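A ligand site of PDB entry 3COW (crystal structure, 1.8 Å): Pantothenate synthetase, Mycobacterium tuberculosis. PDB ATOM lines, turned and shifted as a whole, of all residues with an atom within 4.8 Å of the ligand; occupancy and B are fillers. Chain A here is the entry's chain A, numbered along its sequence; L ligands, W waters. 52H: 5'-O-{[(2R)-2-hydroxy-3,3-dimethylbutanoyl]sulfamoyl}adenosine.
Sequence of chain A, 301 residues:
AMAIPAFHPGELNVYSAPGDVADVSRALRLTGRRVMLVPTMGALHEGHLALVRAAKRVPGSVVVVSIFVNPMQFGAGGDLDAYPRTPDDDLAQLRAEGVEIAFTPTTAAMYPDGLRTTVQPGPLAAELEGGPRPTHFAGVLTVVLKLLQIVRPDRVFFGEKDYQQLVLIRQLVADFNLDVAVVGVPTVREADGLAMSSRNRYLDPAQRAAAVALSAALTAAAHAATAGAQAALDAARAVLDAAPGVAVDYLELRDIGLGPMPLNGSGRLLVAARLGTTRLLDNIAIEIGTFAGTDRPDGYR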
ATOM      1  N   PRO A  39      20.756 -27.578 -22.998  1.00  0.00           N
ATOM      2  CA  PRO A  39      20.245 -28.489 -24.035  1.00  0.00           C
ATOM      3  C   PRO A  39      18.748 -28.317 -24.312  1.00  0.00           C
ATOM      4  O   PRO A  39      17.941 -28.307 -23.363  1.00  0.00           O
ATOM      5  CB  PRO A  39      20.531 -29.882 -23.431  1.00  0.00           C
ATOM      6  CG  PRO A  39      21.634 -29.628 -22.428  1.00  0.00           C
ATOM      7  CD  PRO A  39      21.163 -28.318 -21.798  1.00  0.00           C
ATOM      8  N   THR A  40      18.403 -28.158 -25.583  1.00  0.00           N
ATOM      9  CA  THR A  40      16.983 -28.072 -25.977  1.00  0.00           C
ATOM     10  C   THR A  40      16.721 -28.834 -27.289  1.00  0.00           C
ATOM     11  O   THR A  40      17.664 -29.208 -28.004  1.00  0.00           O
ATOM     12  CB  THR A  40      16.545 -26.575 -26.196  1.00  0.00           C
ATOM     13  OG1 THR A  40      16.906 -26.176 -27.510  1.00  0.00           O
ATOM     14  CG2 THR A  40      17.221 -25.630 -25.184  1.00  0.00           C
ATOM     15  N   MET A  41      15.430 -29.044 -27.588  1.00  0.00           N
ATOM     16  CA  MET A  41      15.002 -29.567 -28.883  1.00  0.00           C
ATOM     17  C   MET A  41      14.280 -28.473 -29.673  1.00  0.00           C
ATOM     18  O   MET A  41      13.451 -28.759 -30.543  1.00  0.00           O
ATOM     19  CB  MET A  41      14.117 -30.814 -28.670  1.00  0.00           C
ATOM     20  CG  MET A  41      14.922 -31.924 -27.993  1.00  0.00           C
ATOM     21  SD  MET A  41      14.368 -33.621 -28.233  1.00  0.00           S
ATOM     22  CE  MET A  41      12.716 -33.584 -27.594  1.00  0.00           C
ATOM     23  N   GLY A  42      14.601 -27.231 -29.373  1.00  0.00           N
ATOM     24  CA  GLY A  42      14.050 -26.075 -30.099  1.00  0.00           C
ATOM     25  C   GLY A  42      12.588 -25.840 -29.781  1.00  0.00           C
ATOM     26  O   GLY A  42      12.050 -26.322 -28.755  1.00  0.00           O
ATOM     27  N   HIS A  45      10.195 -21.611 -25.918  1.00  0.00           N
ATOM     28  CA  HIS A  45       9.224 -20.750 -25.252  1.00  0.00           C
ATOM     29  C   HIS A  45       9.834 -20.238 -23.929  1.00  0.00           C
ATOM     30  O   HIS A  45      10.976 -20.528 -23.615  1.00  0.00           O
ATOM     31  CB  HIS A  45       7.924 -21.534 -25.023  1.00  0.00           C
ATOM     32  CG  HIS A  45       8.122 -22.829 -24.292  1.00  0.00           C
ATOM     33  ND1 HIS A  45       8.537 -22.887 -22.982  1.00  0.00           N
ATOM     34  CD2 HIS A  45       7.976 -24.102 -24.697  1.00  0.00           C
ATOM     35  CE1 HIS A  45       8.628 -24.150 -22.605  1.00  0.00           C
ATOM     36  NE2 HIS A  45       8.280 -24.913 -23.624  1.00  0.00           N
ATOM     37  N   GLY A  47       9.696 -21.046 -20.929  1.00  0.00           N
ATOM     38  CA  GLY A  47      10.236 -22.096 -20.036  1.00  0.00           C
ATOM     39  C   GLY A  47      11.716 -22.378 -20.356  1.00  0.00           C
ATOM     40  O   GLY A  47      12.562 -22.416 -19.444  1.00  0.00           O
ATOM     41  N   HIS A  48      12.025 -22.546 -21.641  1.00  0.00           N
ATOM     42  CA  HIS A  48      13.411 -22.728 -22.118  1.00  0.00           C
ATOM     43  C   HIS A  48      14.200 -21.470 -21.766  1.00  0.00           C
ATOM     44  O   HIS A  48      15.374 -21.552 -21.387  1.00  0.00           O
ATOM     45  CB  HIS A  48      13.454 -22.934 -23.632  1.00  0.00           C
ATOM     46  CG  HIS A  48      12.701 -24.140 -24.112  1.00  0.00           C
ATOM     47  ND1 HIS A  48      11.521 -24.064 -24.822  1.00  0.00           N
ATOM     48  CD2 HIS A  48      12.973 -25.466 -23.985  1.00  0.00           C
ATOM     49  CE1 HIS A  48      11.102 -25.270 -25.122  1.00  0.00           C
ATOM     50  NE2 HIS A  48      11.963 -26.147 -24.620  1.00  0.00           N
ATOM     51  N   LEU A  51      15.857 -21.201 -18.443  1.00  0.00           N
ATOM     52  CA  LEU A  51      17.157 -21.904 -18.315  1.00  0.00           C
ATOM     53  C   LEU A  51      18.248 -21.004 -18.898  1.00  0.00           C
ATOM     54  O   LEU A  51      19.344 -20.934 -18.348  1.00  0.00           O
ATOM     55  CB  LEU A  51      17.155 -23.247 -19.077  1.00  0.00           C
ATOM     56  CG  LEU A  51      16.540 -24.498 -18.435  1.00  0.00           C
ATOM     57  CD1 LEU A  51      15.074 -24.304 -18.020  1.00  0.00           C
ATOM     58  CD2 LEU A  51      16.681 -25.750 -19.341  1.00  0.00           C
ATOM     59  N   GLN A  73      15.504 -40.708 -28.906  1.00  0.00           N
ATOM     60  CA  GLN A  73      14.607 -40.699 -27.742  1.00  0.00           C
ATOM     61  C   GLN A  73      13.125 -40.707 -28.118  1.00  0.00           C
ATOM     62  O   GLN A  73      12.221 -40.609 -27.244  1.00  0.00           O
ATOM     63  CB  GLN A  73      14.945 -39.554 -26.782  1.00  0.00           C
ATOM     64  CG  GLN A  73      14.655 -38.105 -27.340  1.00  0.00           C
ATOM     65  CD  GLN A  73      15.192 -37.008 -26.425  1.00  0.00           C
ATOM     66  OE1 GLN A  73      16.425 -36.868 -26.243  1.00  0.00           O
ATOM     67  NE2 GLN A  73      14.262 -36.233 -25.821  1.00  0.00           N
ATOM     68  N   TYR A  83       7.167 -33.533 -33.941  1.00  0.00           N
ATOM     69  CA  TYR A  83       7.780 -32.588 -33.015  1.00  0.00           C
ATOM     70  C   TYR A  83       7.854 -31.194 -33.649  1.00  0.00           C
ATOM     71  O   TYR A  83       8.307 -31.070 -34.782  1.00  0.00           O
ATOM     72  CB  TYR A  83       9.191 -33.024 -32.597  1.00  0.00           C
ATOM     73  CG  TYR A  83       9.553 -32.369 -31.278  1.00  0.00           C
ATOM     74  CD1 TYR A  83       9.060 -32.883 -30.075  1.00  0.00           C
ATOM     75  CD2 TYR A  83      10.319 -31.204 -31.237  1.00  0.00           C
ATOM     76  CE1 TYR A  83       9.357 -32.264 -28.844  1.00  0.00           C
ATOM     77  CE2 TYR A  83      10.620 -30.584 -30.019  1.00  0.00           C
ATOM     78  CZ  TYR A  83      10.137 -31.121 -28.836  1.00  0.00           C
ATOM     79  OH  TYR A  83      10.435 -30.523 -27.636  1.00  0.00           O
ATOM     80  N   VAL A 140      17.783 -40.007 -24.288  1.00  0.00           N
ATOM     81  CA  VAL A 140      18.057 -38.719 -23.647  1.00  0.00           C
ATOM     82  C   VAL A 140      19.478 -38.733 -23.037  1.00  0.00           C
ATOM     83  O   VAL A 140      20.282 -37.805 -23.247  1.00  0.00           O
ATOM     84  CB  VAL A 140      17.024 -38.441 -22.522  1.00  0.00           C
ATOM     85  CG1 VAL A 140      17.488 -37.238 -21.617  1.00  0.00           C
ATOM     86  CG2 VAL A 140      15.558 -38.270 -23.076  1.00  0.00           C
ATOM     87  N   VAL A 143      22.280 -38.736 -25.736  1.00  0.00           N
ATOM     88  CA  VAL A 143      22.527 -37.452 -26.411  1.00  0.00           C
ATOM     89  C   VAL A 143      23.089 -36.389 -25.448  1.00  0.00           C
ATOM     90  O   VAL A 143      23.945 -35.588 -25.832  1.00  0.00           O
ATOM     91  CB  VAL A 143      21.280 -36.941 -27.210  1.00  0.00           C
ATOM     92  CG1 VAL A 143      20.206 -36.300 -26.249  1.00  0.00           C
ATOM     93  CG2 VAL A 143      21.731 -35.951 -28.354  1.00  0.00           C
ATOM     94  N   VAL A 144      22.668 -36.432 -24.185  1.00  0.00           N
ATOM     95  CA  VAL A 144      23.180 -35.433 -23.245  1.00  0.00           C
ATOM     96  C   VAL A 144      24.662 -35.739 -22.947  1.00  0.00           C
ATOM     97  O   VAL A 144      25.495 -34.815 -22.863  1.00  0.00           O
ATOM     98  CB  VAL A 144      22.322 -35.331 -21.955  1.00  0.00           C
ATOM     99  CG1 VAL A 144      23.094 -34.492 -20.869  1.00  0.00           C
ATOM    100  CG2 VAL A 144      20.978 -34.745 -22.279  1.00  0.00           C
ATOM    101  N   PHE A 157      22.142 -26.998 -17.714  1.00  0.00           N
ATOM    102  CA  PHE A 157      20.884 -26.542 -17.139  1.00  0.00           C
ATOM    103  C   PHE A 157      19.714 -27.400 -17.608  1.00  0.00           C
ATOM    104  O   PHE A 157      19.598 -27.666 -18.807  1.00  0.00           O
ATOM    105  CB  PHE A 157      20.659 -25.065 -17.509  1.00  0.00           C
ATOM    106  CG  PHE A 157      21.643 -24.123 -16.838  1.00  0.00           C
ATOM    107  CD1 PHE A 157      22.968 -24.017 -17.292  1.00  0.00           C
ATOM    108  CD2 PHE A 157      21.267 -23.424 -15.693  1.00  0.00           C
ATOM    109  CE1 PHE A 157      23.899 -23.180 -16.638  1.00  0.00           C
ATOM    110  CE2 PHE A 157      22.190 -22.561 -15.056  1.00  0.00           C
ATOM    111  CZ  PHE A 157      23.507 -22.467 -15.506  1.00  0.00           C
ATOM    112  N   PHE A 158      18.888 -27.847 -16.659  1.00  0.00           N
ATOM    113  CA  PHE A 158      17.713 -28.672 -16.930  1.00  0.00           C
ATOM    114  C   PHE A 158      16.497 -28.140 -16.152  1.00  0.00           C
ATOM    115  O   PHE A 158      16.646 -27.682 -15.017  1.00  0.00           O
ATOM    116  CB  PHE A 158      18.019 -30.119 -16.503  1.00  0.00           C
ATOM    117  CG  PHE A 158      18.825 -30.867 -17.530  1.00  0.00           C
ATOM    118  CD1 PHE A 158      20.213 -30.791 -17.532  1.00  0.00           C
ATOM    119  CD2 PHE A 158      18.174 -31.565 -18.547  1.00  0.00           C
ATOM    120  CE1 PHE A 158      20.946 -31.455 -18.509  1.00  0.00           C
ATOM    121  CE2 PHE A 158      18.896 -32.208 -19.558  1.00  0.00           C
ATOM    122  CZ  PHE A 158      20.280 -32.139 -19.540  1.00  0.00           C
ATOM    123  N   GLY A 159      15.294 -28.233 -16.740  1.00  0.00           N
ATOM    124  CA  GLY A 159      14.083 -27.733 -16.105  1.00  0.00           C
ATOM    125  C   GLY A 159      13.495 -28.751 -15.155  1.00  0.00           C
ATOM    126  O   GLY A 159      13.480 -29.963 -15.429  1.00  0.00           O
ATOM    127  N   GLU A 160      12.963 -28.270 -14.035  1.00  0.00           N
ATOM    128  CA  GLU A 160      12.140 -29.095 -13.165  1.00  0.00           C
ATOM    129  C   GLU A 160      10.876 -29.630 -13.852  1.00  0.00           C
ATOM    130  O   GLU A 160      10.294 -30.600 -13.371  1.00  0.00           O
ATOM    131  CB  GLU A 160      11.788 -28.350 -11.879  1.00  0.00           C
ATOM    132  CG  GLU A 160      13.006 -28.138 -11.000  1.00  0.00           C
ATOM    133  CD  GLU A 160      12.690 -27.515  -9.650  1.00  0.00           C
ATOM    134  OE1 GLU A 160      11.510 -27.460  -9.270  1.00  0.00           O
ATOM    135  OE2 GLU A 160      13.645 -27.082  -8.969  1.00  0.00           O
ATOM    136  N   LYS A 161      10.467 -28.988 -14.965  1.00  0.00           N
ATOM    137  CA  LYS A 161       9.356 -29.461 -15.810  1.00  0.00           C
ATOM    138  C   LYS A 161       9.482 -30.937 -16.120  1.00  0.00           C
ATOM    139  O   LYS A 161       8.515 -31.690 -15.985  1.00  0.00           O
ATOM    140  CB  LYS A 161       9.265 -28.663 -17.132  1.00  0.00           C
ATOM    141  CG  LYS A 161       8.244 -29.234 -18.195  1.00  0.00           C
ATOM    142  CD  LYS A 161       6.887 -28.519 -18.086  1.00  0.00           C
ATOM    143  CE  LYS A 161       5.839 -29.106 -19.031  1.00  0.00           C
ATOM    144  NZ  LYS A 161       5.668 -30.596 -18.767  1.00  0.00           N
ATOM    145  N   ASP A 162      10.691 -31.361 -16.508  1.00  0.00           N
ATOM    146  CA  ASP A 162      10.925 -32.736 -16.809  1.00  0.00           C
ATOM    147  C   ASP A 162      11.732 -33.304 -15.655  1.00  0.00           C
ATOM    148  O   ASP A 162      12.937 -33.496 -15.748  1.00  0.00           O
ATOM    149  CB  ASP A 162      11.646 -32.841 -18.154  1.00  0.00           C
ATOM    150  CG  ASP A 162      10.811 -32.263 -19.257  1.00  0.00           C
ATOM    151  OD1 ASP A 162       9.896 -32.975 -19.718  1.00  0.00           O
ATOM    152  OD2 ASP A 162      10.975 -31.072 -19.572  1.00  0.00           O
ATOM    153  N   GLN A 165      13.579 -36.619 -15.956  1.00  0.00           N
ATOM    154  CA  GLN A 165      14.745 -36.389 -16.776  1.00  0.00           C
ATOM    155  C   GLN A 165      15.893 -35.740 -16.010  1.00  0.00           C
ATOM    156  O   GLN A 165      17.021 -36.194 -16.103  1.00  0.00           O
ATOM    157  CB  GLN A 165      14.372 -35.475 -17.926  1.00  0.00           C
ATOM    158  CG  GLN A 165      15.551 -35.015 -18.725  1.00  0.00           C
ATOM    159  CD  GLN A 165      15.082 -34.342 -19.975  1.00  0.00           C
ATOM    160  OE1 GLN A 165      14.920 -35.005 -20.993  1.00  0.00           O
ATOM    161  NE2 GLN A 165      14.782 -33.040 -19.886  1.00  0.00           N
ATOM    162  N   VAL A 185      16.278 -25.903 -12.835  1.00  0.00           N
ATOM    163  CA  VAL A 185      15.665 -24.585 -12.940  1.00  0.00           C
ATOM    164  C   VAL A 185      14.146 -24.746 -12.711  1.00  0.00           C
ATOM    165  O   VAL A 185      13.551 -25.657 -13.286  1.00  0.00           O
ATOM    166  CB  VAL A 185      15.968 -23.997 -14.301  1.00  0.00           C
ATOM    167  CG1 VAL A 185      15.105 -22.729 -14.570  1.00  0.00           C
ATOM    168  CG2 VAL A 185      17.454 -23.668 -14.401  1.00  0.00           C
ATOM    169  N   PRO A 186      13.531 -23.886 -11.855  1.00  0.00           N
ATOM    170  CA  PRO A 186      12.101 -24.105 -11.577  1.00  0.00           C
ATOM    171  C   PRO A 186      11.170 -24.016 -12.804  1.00  0.00           C
ATOM    172  O   PRO A 186      11.435 -23.272 -13.771  1.00  0.00           O
ATOM    173  CB  PRO A 186      11.764 -22.982 -10.578  1.00  0.00           C
ATOM    174  CG  PRO A 186      13.120 -22.643  -9.944  1.00  0.00           C
ATOM    175  CD  PRO A 186      14.062 -22.726 -11.108  1.00  0.00           C
ATOM    176  N   THR A 187      10.065 -24.741 -12.739  1.00  0.00           N
ATOM    177  CA  THR A 187       9.106 -24.768 -13.851  1.00  0.00           C
ATOM    178  C   THR A 187       8.428 -23.410 -14.126  1.00  0.00           C
ATOM    179  O   THR A 187       7.907 -22.765 -13.209  1.00  0.00           O
ATOM    180  CB  THR A 187       8.041 -25.834 -13.591  1.00  0.00           C
ATOM    181  OG1 THR A 187       8.673 -27.132 -13.561  1.00  0.00           O
ATOM    182  CG2 THR A 187       7.009 -25.816 -14.685  1.00  0.00           C
ATOM    183  N   VAL A 188       8.455 -22.993 -15.383  1.00  0.00           N
ATOM    184  CA  VAL A 188       7.759 -21.762 -15.814  1.00  0.00           C
ATOM    185  C   VAL A 188       6.329 -22.096 -16.165  1.00  0.00           C
ATOM    186  O   VAL A 188       6.065 -23.077 -16.891  1.00  0.00           O
ATOM    187  CB  VAL A 188       8.489 -21.077 -17.000  1.00  0.00           C
ATOM    188  CG1 VAL A 188       7.785 -19.760 -17.333  1.00  0.00           C
ATOM    189  CG2 VAL A 188       9.913 -20.804 -16.608  1.00  0.00           C
ATOM    190  N   ALA A 195       1.821 -25.579 -16.822  1.00  0.00           N
ATOM    191  CA  ALA A 195       3.266 -25.637 -17.058  1.00  0.00           C
ATOM    192  C   ALA A 195       3.496 -25.383 -18.559  1.00  0.00           C
ATOM    193  O   ALA A 195       2.857 -26.013 -19.378  1.00  0.00           O
ATOM    194  CB  ALA A 195       3.799 -27.007 -16.689  1.00  0.00           C
ATOM    195  N   MET A 196       4.432 -24.494 -18.877  1.00  0.00           N
ATOM    196  CA  MET A 196       4.705 -24.208 -20.290  1.00  0.00           C
ATOM    197  C   MET A 196       5.324 -25.404 -20.995  1.00  0.00           C
ATOM    198  O   MET A 196       6.248 -26.049 -20.476  1.00  0.00           O
ATOM    199  CB  MET A 196       5.623 -23.006 -20.400  1.00  0.00           C
ATOM    200  CG  MET A 196       4.878 -21.748 -19.958  1.00  0.00           C
ATOM    201  SD  MET A 196       5.816 -20.304 -20.494  1.00  0.00           S
ATOM    202  CE  MET A 196       5.525 -20.519 -22.235  1.00  0.00           C
HETATM  203  C4  52H L   1      11.389 -26.120 -18.939  1.00  0.00           C
HETATM  204  C5  52H L   1      10.052 -25.837 -19.255  1.00  0.00           C
HETATM  205  C6  52H L   1       9.324 -25.040 -18.364  1.00  0.00           C
HETATM  206  C8  52H L   1      10.873 -27.103 -20.804  1.00  0.00           C
HETATM  207  N1  52H L   1       9.981 -24.549 -17.297  1.00  0.00           N
HETATM  208  N3  52H L   1      11.976 -25.610 -17.824  1.00  0.00           N
HETATM  209  CAA 52H L   1      17.732 -34.125 -24.758  1.00  0.00           C
HETATM  210  CBB 52H L   1      16.979 -32.915 -24.198  1.00  0.00           C
HETATM  211  CAB 52H L   1      17.468 -31.686 -24.953  1.00  0.00           C
HETATM  212  CAC 52H L   1      17.291 -32.852 -22.728  1.00  0.00           C
HETATM  213  CAX 52H L   1      15.439 -33.114 -24.337  1.00  0.00           C
HETATM  214  OAH 52H L   1      14.984 -34.344 -23.691  1.00  0.00           O
HETATM  215  CAT 52H L   1      14.527 -31.976 -23.799  1.00  0.00           C
HETATM  216  OAE 52H L   1      14.005 -32.042 -22.677  1.00  0.00           O
HETATM  217  NAQ 52H L   1      14.304 -31.023 -24.682  1.00  0.00           N
HETATM  218  SBE 52H L   1      13.270 -29.792 -24.433  1.00  0.00           S
HETATM  219  OAF 52H L   1      11.874 -30.284 -24.371  1.00  0.00           O
HETATM  220  OAG 52H L   1      13.509 -28.774 -25.471  1.00  0.00           O
HETATM  221  O5' 52H L   1      13.448 -29.143 -23.142  1.00  0.00           O
HETATM  222  C5' 52H L   1      14.751 -28.475 -22.946  1.00  0.00           C
HETATM  223  C4' 52H L   1      14.947 -28.073 -21.458  1.00  0.00           C
HETATM  224  O4' 52H L   1      13.962 -27.052 -21.166  1.00  0.00           O
HETATM  225  C3' 52H L   1      14.652 -29.247 -20.532  1.00  0.00           C
HETATM  226  O3' 52H L   1      15.595 -29.239 -19.473  1.00  0.00           O
HETATM  227  C2' 52H L   1      13.238 -28.943 -20.017  1.00  0.00           C
HETATM  228  O2' 52H L   1      12.940 -29.470 -18.697  1.00  0.00           O
HETATM  229  C1' 52H L   1      13.259 -27.416 -19.951  1.00  0.00           C
HETATM  230  N9  52H L   1      11.872 -26.892 -19.906  1.00  0.00           N
HETATM  231  N7  52H L   1       9.746 -26.455 -20.406  1.00  0.00           N
HETATM  232  C2  52H L   1      11.248 -24.842 -17.010  1.00  0.00           C
HETATM  233  N6  52H L   1       8.035 -24.742 -18.607  1.00  0.00           N
HETATM  234  O   HOH W   1      11.039 -32.864 -22.846  1.00  0.00           O
HETATM  235  O   HOH W   2      14.785 -31.783 -17.205  1.00  0.00           O
HETATM  236  O   HOH W   3      10.642 -27.951 -26.928  1.00  0.00           O
HETATM  237  O   HOH W   4      17.958 -28.933 -20.669  1.00  0.00           O
HETATM  238  O   HOH W   5      10.228 -30.185 -21.950  1.00  0.00           O
HETATM  239  O   HOH W   6      10.179 -32.662 -25.261  1.00  0.00           O
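An oxygen (OAH) of the ligand lies within hydrogen-bond range of the side-chain amide nitrogen (NE2) of Gln 73, at 2.9 Å. O of Val 188 is in hydrogen-bond range of N6 of the ligand, 3.1 Å away. The side-chain carboxylate of Asp 162 lies within hydrogen-bond range of an oxygen (O2') of the ligand, at 2.7 Å. An oxygen (OAG) of the ligand sits at hydrogen-bond distance from the backbone NH (N) of Met 41 (2.9 Å). An oxygen (OAG) of the ligand is in hydrogen-bond range of a ring nitrogen (NE2) of His 48 (3.2 Å). O of Met 196 is in hydrogen-bond range of N6 of the ligand (2.9 Å). The backbone NH (N) of Gly 159 is in hydrogen-bond range of an oxygen (O3') of the ligand. The side-chain amide oxygen of Gln 165 is in hydrogen-bond range of an oxygen (OAH) of the ligand, 2.8 Å away. O of Gly 159 sits close to O2' of the ligand, 3.3 Å away. The backbone NH (N) of Val 188 is in hydrogen-bond range of a nitrogen (N1) of the ligand (2.9 Å).
SD of Met 41 lies close to NE2 of Gln 73 (3.6 Å). N of Met 196 lies within hydrogen-bond range of O of Val 188 (2.9 Å). The backbone NH (N) of Gly 42 lies within hydrogen-bond range of the side-chain hydroxyl (OG1) of Thr 40, 3.1 Å away. N of Gly 47 lies within hydrogen-bond range of ND1 of His 45. N of Val 185 lies within hydrogen-bond range of O of Phe 158, at 2.8 Å. The backbone NH of His 45 is in hydrogen-bond range of a ring nitrogen (ND1) of His 48 (3.0 Å). The side-chain hydroxyl (OG1) of Thr 187 lies within hydrogen-bond range of the backbone NH (N) of Lys 161, 2.9 Å away.
O of Pro 39 touches C5' of the ligand, at 3.2 Å. Thr 40 touches the ligand (CA to OAG, 3.6 Å). His 45 touches the ligand. Gly 47 touches the ligand. Leu 51 touches the ligand. Tyr 83 touches the ligand. CG1 of Val 143 touches CAA of the ligand, at 3.6 Å. Phe 158 touches the ligand. Lys 161 touches the ligand (CB to C5, 3.6 Å). Pro 186 touches the ligand (O to C2, 3.6 Å). CA of Thr 187 touches N1 of the ligand (3.6 Å). Hydrophobic or aromatic side chains within 4 Å of the ligand: Pro 39, Met 41, His 45, His 48, Leu 51, Val 143, Phe 158, Val 188 and Met 196. The nearest printed residue that does not touch the ligand is Val 140 (4.02 Å).
Water W4 lies within hydrogen-bond range of O3' of the ligand, O of Pro 39 and O of Phe 157. Water W5 lies within hydrogen-bond range of the side-chain carboxylate of Asp 162 (2.6 Å) and an oxygen (OAF) of the ligand (2.9 Å). Water W6 lies within hydrogen-bond range of OAF of the ligand (3.1 Å) and OH of Tyr 83 (3.2 Å). Water W1 lies within hydrogen-bond range of OAE of the ligand (3.1 Å) and OD1 of Asp 162 (3.3 Å). Water W2 lies within hydrogen-bond range of the backbone carbonyl oxygen of Gly 159, the backbone carbonyl oxygen of Asp 162, the side-chain amide nitrogen of Gln 165 and an oxygen (O2') of the ligand. Water W3 lies within hydrogen-bond range of OH of Tyr 83 (2.7 Å), O of Gly 42 (2.8 Å), NE2 of His 48 (3.2 Å) and OAG of the ligand (3.3 Å).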
